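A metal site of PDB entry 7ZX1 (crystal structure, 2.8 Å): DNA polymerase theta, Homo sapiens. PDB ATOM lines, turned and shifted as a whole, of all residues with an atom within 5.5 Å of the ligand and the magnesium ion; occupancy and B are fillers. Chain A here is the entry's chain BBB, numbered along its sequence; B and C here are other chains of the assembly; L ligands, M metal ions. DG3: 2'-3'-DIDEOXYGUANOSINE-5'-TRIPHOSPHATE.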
ATOM      1  N   ARG A 422      18.828  34.052  26.122  1.00  0.00           N
ATOM      2  CA  ARG A 422      18.746  33.718  27.550  1.00  0.00           C
ATOM      3  C   ARG A 422      19.012  34.969  28.369  1.00  0.00           C
ATOM      4  O   ARG A 422      19.637  35.919  27.873  1.00  0.00           O
ATOM      5  CB  ARG A 422      19.760  32.642  27.936  1.00  0.00           C
ATOM      6  CG  ARG A 422      19.373  31.245  27.481  1.00  0.00           C
ATOM      7  CD  ARG A 422      20.189  30.200  28.178  1.00  0.00           C
ATOM      8  NE  ARG A 422      19.602  28.880  28.107  1.00  0.00           N
ATOM      9  CZ  ARG A 422      20.049  27.832  28.788  1.00  0.00           C
ATOM     10  NH1 ARG A 422      21.097  27.960  29.593  1.00  0.00           N
ATOM     11  NH2 ARG A 422      19.441  26.661  28.654  1.00  0.00           N
ATOM     12  N   ARG A 435      23.064  22.908  43.071  1.00  0.00           N
ATOM     13  CA  ARG A 435      22.032  21.877  43.390  1.00  0.00           C
ATOM     14  C   ARG A 435      22.389  21.302  44.765  1.00  0.00           C
ATOM     15  O   ARG A 435      23.610  21.346  45.128  1.00  0.00           O
ATOM     16  CB  ARG A 435      22.058  20.779  42.321  1.00  0.00           C
ATOM     17  CG  ARG A 435      21.729  21.273  40.912  1.00  0.00           C
ATOM     18  CD  ARG A 435      21.987  20.258  39.834  1.00  0.00           C
ATOM     19  NE  ARG A 435      20.966  19.222  39.839  1.00  0.00           N
ATOM     20  CZ  ARG A 435      19.710  19.357  39.416  1.00  0.00           C
ATOM     21  NH1 ARG A 435      18.885  18.333  39.498  1.00  0.00           N
ATOM     22  NH2 ARG A 435      19.291  20.515  38.932  1.00  0.00           N
ATOM     23  N   ASP A 466       8.671  25.087  36.228  1.00  0.00           N
ATOM     24  CA  ASP A 466       9.742  24.645  35.315  1.00  0.00           C
ATOM     25  C   ASP A 466       9.089  23.964  34.104  1.00  0.00           C
ATOM     26  O   ASP A 466       8.090  23.247  34.244  1.00  0.00           O
ATOM     27  CB  ASP A 466      10.697  23.739  36.124  1.00  0.00           C
ATOM     28  CG  ASP A 466      11.429  22.647  35.376  1.00  0.00           C
ATOM     29  OD1 ASP A 466      10.892  21.509  35.302  1.00  0.00           O
ATOM     30  OD2 ASP A 466      12.572  22.919  34.898  1.00  0.00           O
ATOM     31  N   TYR A 467       9.595  24.198  32.921  1.00  0.00           N
ATOM     32  CA  TYR A 467       9.265  23.470  31.686  1.00  0.00           C
ATOM     33  C   TYR A 467      10.007  22.121  31.727  1.00  0.00           C
ATOM     34  O   TYR A 467      11.172  21.972  32.256  1.00  0.00           O
ATOM     35  CB  TYR A 467       9.633  24.272  30.420  1.00  0.00           C
ATOM     36  CG  TYR A 467       8.709  25.405  30.050  1.00  0.00           C
ATOM     37  CD1 TYR A 467       7.400  25.164  29.678  1.00  0.00           C
ATOM     38  CD2 TYR A 467       9.140  26.718  29.990  1.00  0.00           C
ATOM     39  CE1 TYR A 467       6.535  26.182  29.301  1.00  0.00           C
ATOM     40  CE2 TYR A 467       8.294  27.751  29.610  1.00  0.00           C
ATOM     41  CZ  TYR A 467       6.992  27.476  29.263  1.00  0.00           C
ATOM     42  OH  TYR A 467       6.152  28.492  28.889  1.00  0.00           O
ATOM     43  N   SER A 468       9.291  21.103  31.268  1.00  0.00           N
ATOM     44  CA  SER A 468       9.765  19.701  31.213  1.00  0.00           C
ATOM     45  C   SER A 468      10.227  19.464  29.763  1.00  0.00           C
ATOM     46  O   SER A 468       9.371  19.282  28.877  1.00  0.00           O
ATOM     47  CB  SER A 468       8.688  18.720  31.658  1.00  0.00           C
ATOM     48  OG  SER A 468       7.911  19.228  32.745  1.00  0.00           O
ATOM     49  N   GLN A 469      11.549  19.477  29.584  1.00  0.00           N
ATOM     50  CA  GLN A 469      12.193  19.181  28.274  1.00  0.00           C
ATOM     51  C   GLN A 469      11.632  20.143  27.254  1.00  0.00           C
ATOM     52  O   GLN A 469      11.218  19.685  26.177  1.00  0.00           O
ATOM     53  CB  GLN A 469      11.986  17.722  27.888  1.00  0.00           C
ATOM     54  CG  GLN A 469      12.677  16.728  28.819  1.00  0.00           C
ATOM     55  CD  GLN A 469      11.763  16.216  29.898  1.00  0.00           C
ATOM     56  OE1 GLN A 469      10.662  15.755  29.624  1.00  0.00           O
ATOM     57  NE2 GLN A 469      12.224  16.302  31.135  1.00  0.00           N
ATOM     58  N   LEU A 470      11.759  21.454  27.508  1.00  0.00           N
ATOM     59  CA  LEU A 470      11.267  22.483  26.556  1.00  0.00           C
ATOM     60  C   LEU A 470      12.051  22.371  25.263  1.00  0.00           C
ATOM     61  O   LEU A 470      11.426  22.379  24.196  1.00  0.00           O
ATOM     62  CB  LEU A 470      11.393  23.878  27.187  1.00  0.00           C
ATOM     63  CG  LEU A 470      10.840  25.026  26.349  1.00  0.00           C
ATOM     64  CD1 LEU A 470       9.396  24.765  25.950  1.00  0.00           C
ATOM     65  CD2 LEU A 470      10.952  26.342  27.084  1.00  0.00           C
ATOM     66  N   GLU A 471      13.383  22.259  25.355  1.00  0.00           N
ATOM     67  CA  GLU A 471      14.274  22.174  24.169  1.00  0.00           C
ATOM     68  C   GLU A 471      13.945  20.917  23.358  1.00  0.00           C
ATOM     69  O   GLU A 471      13.995  20.998  22.126  1.00  0.00           O
ATOM     70  CB  GLU A 471      15.746  22.318  24.589  1.00  0.00           C
ATOM     71  CG  GLU A 471      16.216  23.778  24.536  1.00  0.00           C
ATOM     72  CD  GLU A 471      17.577  24.147  25.135  1.00  0.00           C
ATOM     73  OE1 GLU A 471      18.605  23.715  24.582  1.00  0.00           O
ATOM     74  OE2 GLU A 471      17.576  24.920  26.135  1.00  0.00           O
ATOM     75  N   ASP A 493      10.416   9.400  32.019  1.00  0.00           N
ATOM     76  CA  ASP A 493      11.493  10.430  31.945  1.00  0.00           C
ATOM     77  C   ASP A 493      12.625   9.906  31.057  1.00  0.00           C
ATOM     78  O   ASP A 493      13.155   8.809  31.356  1.00  0.00           O
ATOM     79  CB  ASP A 493      12.000  10.816  33.339  1.00  0.00           C
ATOM     80  CG  ASP A 493      12.833  12.081  33.341  1.00  0.00           C
ATOM     81  OD1 ASP A 493      12.398  13.087  32.782  1.00  0.00           O
ATOM     82  OD2 ASP A 493      13.934  12.047  33.914  1.00  0.00           O
ATOM     83  N   PHE A 495      15.662  10.940  30.563  1.00  0.00           N
ATOM     84  CA  PHE A 495      16.967  10.895  31.266  1.00  0.00           C
ATOM     85  C   PHE A 495      17.044   9.605  32.107  1.00  0.00           C
ATOM     86  O   PHE A 495      18.094   8.925  32.036  1.00  0.00           O
ATOM     87  CB  PHE A 495      17.197  12.208  32.011  1.00  0.00           C
ATOM     88  CG  PHE A 495      16.966  13.434  31.161  1.00  0.00           C
ATOM     89  CD1 PHE A 495      17.554  13.547  29.904  1.00  0.00           C
ATOM     90  CD2 PHE A 495      16.156  14.462  31.603  1.00  0.00           C
ATOM     91  CE1 PHE A 495      17.326  14.664  29.118  1.00  0.00           C
ATOM     92  CE2 PHE A 495      15.941  15.583  30.821  1.00  0.00           C
ATOM     93  CZ  PHE A 495      16.529  15.682  29.583  1.00  0.00           C
ATOM     94  N   ARG A 515      21.010  11.131  37.083  1.00  0.00           N
ATOM     95  CA  ARG A 515      19.998  11.668  36.120  1.00  0.00           C
ATOM     96  C   ARG A 515      20.590  12.882  35.393  1.00  0.00           C
ATOM     97  O   ARG A 515      20.370  12.989  34.171  1.00  0.00           O
ATOM     98  CB  ARG A 515      18.687  12.058  36.817  1.00  0.00           C
ATOM     99  CG  ARG A 515      17.594  12.475  35.840  1.00  0.00           C
ATOM    100  CD  ARG A 515      16.253  12.602  36.510  1.00  0.00           C
ATOM    101  NE  ARG A 515      15.263  13.177  35.603  1.00  0.00           N
ATOM    102  CZ  ARG A 515      15.126  14.474  35.358  1.00  0.00           C
ATOM    103  NH1 ARG A 515      14.183  14.888  34.519  1.00  0.00           N
ATOM    104  NH2 ARG A 515      15.921  15.358  35.931  1.00  0.00           N
ATOM    105  N   GLN A 516      21.347  13.722  36.100  1.00  0.00           N
ATOM    106  CA  GLN A 516      22.110  14.869  35.532  1.00  0.00           C
ATOM    107  C   GLN A 516      23.162  14.348  34.535  1.00  0.00           C
ATOM    108  O   GLN A 516      23.265  14.948  33.447  1.00  0.00           O
ATOM    109  CB  GLN A 516      22.768  15.676  36.657  1.00  0.00           C
ATOM    110  CG  GLN A 516      21.761  16.302  37.596  1.00  0.00           C
ATOM    111  CD  GLN A 516      20.987  17.406  36.934  1.00  0.00           C
ATOM    112  OE1 GLN A 516      19.872  17.209  36.444  1.00  0.00           O
ATOM    113  NE2 GLN A 516      21.588  18.584  36.901  1.00  0.00           N
ATOM    114  N   LYS A 519      21.218  13.437  31.481  1.00  0.00           N
ATOM    115  CA  LYS A 519      20.735  14.712  30.884  1.00  0.00           C
ATOM    116  C   LYS A 519      21.861  15.268  29.990  1.00  0.00           C
ATOM    117  O   LYS A 519      21.561  15.591  28.831  1.00  0.00           O
ATOM    118  CB  LYS A 519      20.355  15.689  31.999  1.00  0.00           C
ATOM    119  CG  LYS A 519      19.925  17.081  31.562  1.00  0.00           C
ATOM    120  CD  LYS A 519      19.424  17.908  32.707  1.00  0.00           C
ATOM    121  CE  LYS A 519      18.068  17.463  33.206  1.00  0.00           C
ATOM    122  NZ  LYS A 519      17.596  18.300  34.322  1.00  0.00           N
ATOM    123  N   GLN A 520      23.095  15.315  30.513  1.00  0.00           N
ATOM    124  CA  GLN A 520      24.301  15.841  29.813  1.00  0.00           C
ATOM    125  C   GLN A 520      24.532  14.999  28.555  1.00  0.00           C
ATOM    126  O   GLN A 520      24.847  15.567  27.497  1.00  0.00           O
ATOM    127  CB  GLN A 520      25.547  15.750  30.696  1.00  0.00           C
ATOM    128  CG  GLN A 520      26.012  17.090  31.265  1.00  0.00           C
ATOM    129  CD  GLN A 520      27.509  17.091  31.469  1.00  0.00           C
ATOM    130  OE1 GLN A 520      28.284  17.435  30.580  1.00  0.00           O
ATOM    131  NE2 GLN A 520      27.943  16.622  32.628  1.00  0.00           N
ATOM    132  N   TYR A 523      21.386  15.752  25.784  1.00  0.00           N
ATOM    133  CA  TYR A 523      21.549  17.087  25.138  1.00  0.00           C
ATOM    134  C   TYR A 523      22.898  17.139  24.402  1.00  0.00           C
ATOM    135  O   TYR A 523      22.941  17.690  23.292  1.00  0.00           O
ATOM    136  CB  TYR A 523      21.358  18.214  26.157  1.00  0.00           C
ATOM    137  CG  TYR A 523      19.932  18.395  26.611  1.00  0.00           C
ATOM    138  CD1 TYR A 523      18.929  18.653  25.696  1.00  0.00           C
ATOM    139  CD2 TYR A 523      19.585  18.297  27.945  1.00  0.00           C
ATOM    140  CE1 TYR A 523      17.617  18.822  26.105  1.00  0.00           C
ATOM    141  CE2 TYR A 523      18.273  18.473  28.376  1.00  0.00           C
ATOM    142  CZ  TYR A 523      17.283  18.730  27.443  1.00  0.00           C
ATOM    143  OH  TYR A 523      15.977  18.896  27.840  1.00  0.00           O
ATOM    144  N   GLY A 524      23.946  16.558  24.976  1.00  0.00           N
ATOM    145  CA  GLY A 524      25.287  16.483  24.365  1.00  0.00           C
ATOM    146  C   GLY A 524      25.223  15.865  22.972  1.00  0.00           C
ATOM    147  O   GLY A 524      25.642  16.528  21.966  1.00  0.00           O
ATOM    148  N   TYR A 527      23.298  17.920  20.397  1.00  0.00           N
ATOM    149  CA  TYR A 527      23.917  19.211  19.967  1.00  0.00           C
ATOM    150  C   TYR A 527      25.330  18.958  19.445  1.00  0.00           C
ATOM    151  O   TYR A 527      26.110  19.936  19.371  1.00  0.00           O
ATOM    152  CB  TYR A 527      23.827  20.251  21.091  1.00  0.00           C
ATOM    153  CG  TYR A 527      22.422  20.710  21.401  1.00  0.00           C
ATOM    154  CD1 TYR A 527      21.606  21.276  20.434  1.00  0.00           C
ATOM    155  CD2 TYR A 527      21.890  20.600  22.679  1.00  0.00           C
ATOM    156  CE1 TYR A 527      20.303  21.677  20.704  1.00  0.00           C
ATOM    157  CE2 TYR A 527      20.597  21.000  22.969  1.00  0.00           C
ATOM    158  CZ  TYR A 527      19.797  21.542  21.982  1.00  0.00           C
ATOM    159  OH  TYR A 527      18.520  21.938  22.279  1.00  0.00           O
ATOM    160  N   ASN A 606      21.880  24.547  17.751  1.00  0.00           N
ATOM    161  CA  ASN A 606      21.603  24.835  19.178  1.00  0.00           C
ATOM    162  C   ASN A 606      20.931  26.204  19.324  1.00  0.00           C
ATOM    163  O   ASN A 606      20.059  26.347  20.210  1.00  0.00           O
ATOM    164  CB  ASN A 606      22.889  24.762  20.012  1.00  0.00           C
ATOM    165  CG  ASN A 606      22.695  25.203  21.448  1.00  0.00           C
ATOM    166  OD1 ASN A 606      23.212  26.254  21.835  1.00  0.00           O
ATOM    167  ND2 ASN A 606      21.970  24.421  22.240  1.00  0.00           N
ATOM    168  N   GLN A 610      17.599  26.459  21.569  1.00  0.00           N
ATOM    169  CA  GLN A 610      17.837  27.155  22.860  1.00  0.00           C
ATOM    170  C   GLN A 610      17.272  28.576  22.766  1.00  0.00           C
ATOM    171  O   GLN A 610      16.667  29.016  23.750  1.00  0.00           O
ATOM    172  CB  GLN A 610      19.331  27.178  23.197  1.00  0.00           C
ATOM    173  CG  GLN A 610      19.643  27.751  24.574  1.00  0.00           C
ATOM    174  CD  GLN A 610      21.123  27.800  24.870  1.00  0.00           C
ATOM    175  OE1 GLN A 610      21.722  28.859  24.977  1.00  0.00           O
ATOM    176  NE2 GLN A 610      21.713  26.631  24.998  1.00  0.00           N
ATOM    177  N   ASP A 676      14.626  27.850  31.993  1.00  0.00           N
ATOM    178  CA  ASP A 676      13.353  27.167  31.652  1.00  0.00           C
ATOM    179  C   ASP A 676      12.447  27.183  32.877  1.00  0.00           C
ATOM    180  O   ASP A 676      11.478  26.404  32.903  1.00  0.00           O
ATOM    181  CB  ASP A 676      13.601  25.745  31.168  1.00  0.00           C
ATOM    182  CG  ASP A 676      13.971  24.773  32.276  1.00  0.00           C
ATOM    183  OD1 ASP A 676      14.548  25.216  33.314  1.00  0.00           O
ATOM    184  OD2 ASP A 676      13.675  23.592  32.106  1.00  0.00           O
ATOM    185  P    DC B   3      32.973  17.716  21.676  1.00  0.00           P
ATOM    186  OP1  DC B   3      33.679  18.101  22.972  1.00  0.00           O
ATOM    187  OP2  DC B   3      32.940  16.245  21.316  1.00  0.00           O
ATOM    188  O5'  DC B   3      31.436  18.185  21.753  1.00  0.00           O
ATOM    189  C5'  DC B   3      31.124  19.556  22.050  1.00  0.00           C
ATOM    190  C4'  DC B   3      29.696  19.811  21.657  1.00  0.00           C
ATOM    191  O4'  DC B   3      28.834  18.923  22.393  1.00  0.00           O
ATOM    192  C3'  DC B   3      29.181  21.213  21.944  1.00  0.00           C
ATOM    193  O3'  DC B   3      29.365  22.027  20.789  1.00  0.00           O
ATOM    194  C2'  DC B   3      27.694  20.987  22.204  1.00  0.00           C
ATOM    195  C1'  DC B   3      27.647  19.573  22.766  1.00  0.00           C
ATOM    196  N1   DC B   3      27.543  19.494  24.247  1.00  0.00           N
ATOM    197  C2   DC B   3      26.338  19.853  24.853  1.00  0.00           C
ATOM    198  O2   DC B   3      25.406  20.260  24.145  1.00  0.00           O
ATOM    199  N3   DC B   3      26.218  19.751  26.185  1.00  0.00           N
ATOM    200  C4   DC B   3      27.251  19.323  26.931  1.00  0.00           C
ATOM    201  N4   DC B   3      27.054  19.252  28.233  1.00  0.00           N
ATOM    202  C5   DC B   3      28.481  18.946  26.347  1.00  0.00           C
ATOM    203  C6   DC B   3      28.586  19.052  25.007  1.00  0.00           C
ATOM    204  P    DC B   4      30.134  23.393  21.117  1.00  0.00           P
ATOM    205  OP1  DC B   4      30.660  24.061  19.858  1.00  0.00           O
ATOM    206  OP2  DC B   4      31.140  23.268  22.253  1.00  0.00           O
ATOM    207  O5'  DC B   4      28.884  24.259  21.628  1.00  0.00           O
ATOM    208  C5'  DC B   4      27.879  24.624  20.674  1.00  0.00           C
ATOM    209  C4'  DC B   4      26.681  25.180  21.395  1.00  0.00           C
ATOM    210  O4'  DC B   4      26.194  24.205  22.332  1.00  0.00           O
ATOM    211  C3'  DC B   4      26.947  26.430  22.214  1.00  0.00           C
ATOM    212  O3'  DC B   4      26.647  27.600  21.457  1.00  0.00           O
ATOM    213  C2'  DC B   4      25.932  26.352  23.331  1.00  0.00           C
ATOM    214  C1'  DC B   4      25.588  24.868  23.423  1.00  0.00           C
ATOM    215  N1   DC B   4      26.072  24.250  24.680  1.00  0.00           N
ATOM    216  C2   DC B   4      25.233  24.325  25.788  1.00  0.00           C
ATOM    217  O2   DC B   4      24.142  24.877  25.653  1.00  0.00           O
ATOM    218  N3   DC B   4      25.626  23.767  26.949  1.00  0.00           N
ATOM    219  C4   DC B   4      26.822  23.189  27.039  1.00  0.00           C
ATOM    220  N4   DC B   4      27.159  22.673  28.216  1.00  0.00           N
ATOM    221  C5   DC B   4      27.713  23.142  25.930  1.00  0.00           C
ATOM    222  C6   DC B   4      27.302  23.685  24.773  1.00  0.00           C
ATOM    223  P   DDG C  13      20.677  23.600  37.596  1.00  0.00           P
ATOM    224  OP1 DDG C  13      19.440  23.557  38.445  1.00  0.00           O
ATOM    225  OP2 DDG C  13      21.450  22.354  37.263  1.00  0.00           O
ATOM    226  O5' DDG C  13      20.409  24.332  36.176  1.00  0.00           O
ATOM    227  C5' DDG C  13      19.346  25.232  36.064  1.00  0.00           C
ATOM    228  C4' DDG C  13      19.338  25.798  34.659  1.00  0.00           C
ATOM    229  O4' DDG C  13      20.641  26.007  34.166  1.00  0.00           O
ATOM    230  C3' DDG C  13      18.682  24.807  33.706  1.00  0.00           C
ATOM    231  C2' DDG C  13      19.426  25.000  32.403  1.00  0.00           C
ATOM    232  C1' DDG C  13      20.712  25.721  32.780  1.00  0.00           C
ATOM    233  N9  DDG C  13      21.876  24.865  32.504  1.00  0.00           N
ATOM    234  C8  DDG C  13      22.499  24.065  33.359  1.00  0.00           C
ATOM    235  N7  DDG C  13      23.564  23.481  32.745  1.00  0.00           N
ATOM    236  C5  DDG C  13      23.590  23.878  31.491  1.00  0.00           C
ATOM    237  C6  DDG C  13      24.453  23.658  30.323  1.00  0.00           C
ATOM    238  O6  DDG C  13      25.410  22.895  30.356  1.00  0.00           O
ATOM    239  N1  DDG C  13      24.177  24.330  29.223  1.00  0.00           N
ATOM    240  C2  DDG C  13      23.148  25.199  29.146  1.00  0.00           C
ATOM    241  N2  DDG C  13      22.950  25.857  27.995  1.00  0.00           N
ATOM    242  N3  DDG C  13      22.313  25.448  30.179  1.00  0.00           N
ATOM    243  C4  DDG C  13      22.509  24.832  31.359  1.00  0.00           C
HETATM  244  PG  DG3 L   1      14.229  18.562  34.035  1.00  0.00           P
HETATM  245  O1G DG3 L   1      15.143  17.874  35.006  1.00  0.00           O
HETATM  246  O2G DG3 L   1      13.801  19.969  34.450  1.00  0.00           O
HETATM  247  O3G DG3 L   1      13.030  17.713  33.658  1.00  0.00           O
HETATM  248  O3B DG3 L   1      15.210  18.692  32.778  1.00  0.00           O
HETATM  249  PB  DG3 L   1      15.247  19.631  31.483  1.00  0.00           P
HETATM  250  O1B DG3 L   1      15.413  18.817  30.239  1.00  0.00           O
HETATM  251  O2B DG3 L   1      14.167  20.678  31.557  1.00  0.00           O
HETATM  252  O3A DG3 L   1      16.681  20.298  31.690  1.00  0.00           O
HETATM  253  PA  DG3 L   1      16.916  21.460  32.732  1.00  0.00           P
HETATM  254  O1A DG3 L   1      17.944  20.928  33.661  1.00  0.00           O
HETATM  255  O2A DG3 L   1      15.534  21.889  33.190  1.00  0.00           O
HETATM  256  O5' DG3 L   1      17.644  22.499  31.755  1.00  0.00           O
HETATM  257  C5' DG3 L   1      16.826  23.239  30.812  1.00  0.00           C
HETATM  258  C4' DG3 L   1      17.344  23.124  29.374  1.00  0.00           C
HETATM  259  O4' DG3 L   1      18.671  23.665  29.248  1.00  0.00           O
HETATM  260  C3' DG3 L   1      17.474  21.728  28.823  1.00  0.00           C
HETATM  261  C2' DG3 L   1      18.382  21.964  27.653  1.00  0.00           C
HETATM  262  C1' DG3 L   1      19.378  22.943  28.248  1.00  0.00           C
HETATM  263  N9  DG3 L   1      20.503  22.254  28.853  1.00  0.00           N
HETATM  264  C8  DG3 L   1      20.577  21.748  30.116  1.00  0.00           C
HETATM  265  N7  DG3 L   1      21.708  21.123  30.353  1.00  0.00           N
HETATM  266  C5  DG3 L   1      22.401  21.191  29.156  1.00  0.00           C
HETATM  267  C6  DG3 L   1      23.660  20.685  28.813  1.00  0.00           C
HETATM  268  O6  DG3 L   1      24.435  20.015  29.514  1.00  0.00           O
HETATM  269  N1  DG3 L   1      23.996  20.983  27.494  1.00  0.00           N
HETATM  270  C2  DG3 L   1      23.205  21.674  26.611  1.00  0.00           C
HETATM  271  N2  DG3 L   1      23.711  21.827  25.384  1.00  0.00           N
HETATM  272  N3  DG3 L   1      22.007  22.161  26.936  1.00  0.00           N
HETATM  273  C4  DG3 L   1      21.673  21.885  28.220  1.00  0.00           C
HETATM  274 MG    MG M   1      13.439  21.621  33.223  1.00  0.00          MG
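Of the 23 residues printed, 3 come within 4 Å of the magnesium ion. Along chain A the residues within 4 Å of the magnesium ion span positions 466 to 676.
O6 of DDG 13 of chain C sits close to O6 of the ligand (3.2 Å). Residues that only touch the ligand: Phe 495, Glu 471, Tyr 527 and Gln 520. Hydrophobic or aromatic side chains that line the ligand: Phe 495, Tyr 523 and Tyr 527. Within 4 Å of the ligand: Arg 422, Asp 466, Tyr 467, Gln 469, Glu 471, Phe 495, Arg 515, Lys 519, Gln 520, Tyr 523, Tyr 527, Asp 676, DC 3 of chain B, DC 4 of chain B and DDG 13 of chain C. The nearest printed residue that does not touch the ligand is Asn 606 (4.4 Å).
The magnesium ion is bound by O2B of the ligand, O2G of the ligand, O2A of the ligand, OD2 of Asp 676, OD2 of Asp 466 and O of Tyr 467. The magnesium ion has six donor atoms within binding distance.
O2B of the ligand sits close to N of Gln 469 (3.5 Å). O2 of DC 4 of chain B lies close to a nitrogen (N2) of the ligand (3.1 Å). OH of Tyr 523 is in hydrogen-bond range of O1B of the ligand (2.5 Å). NH2 of Arg 422 is in hydrogen-bond range of O4' of the ligand, 3.1 Å away. The side-chain amide nitrogen of Gln 469 lies within hydrogen-bond range of an oxygen (O3G) of the ligand (3.0 Å). N2 of the ligand is in hydrogen-bond range of O2 of DC 3 of chain B (2.6 Å). The side-chain amino group of Lys 519 is in salt-bridge range of an oxygen (O1G) of the ligand. The guanidinium group (NH2) of Arg 515 is in salt-bridge range of an oxygen (O1G) of the ligand (2.8 Å).
N4 of DC 3 of chain B sits close to OE1 of Gln 520. N3 of DDG 13 of chain C lies within hydrogen-bond range of NH1 of Arg 422 (2.9 Å). OP1 of DDG 13 of chain C is in salt-bridge range of the guanidinium group (NH2) of Arg 435 (3.1 Å). The guanidinium group (NH2) of Arg 422 lies within salt-bridge range of the side-chain carboxylate (OE2) of Glu 471, 3.6 Å away. O2 of DC 4 of chain B sits at hydrogen-bond distance from NE2 of Gln 610 (3.1 Å). NZ of Lys 519 is in hydrogen-bond range of OE1 of Gln 516 (3.3 Å). N2 of DDG 13 of chain C sits at hydrogen-bond distance from NE2 of Gln 610 (3.3 Å). OD2 of Asp 493 is in salt-bridge range of NE of Arg 515, 2.4 Å away.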
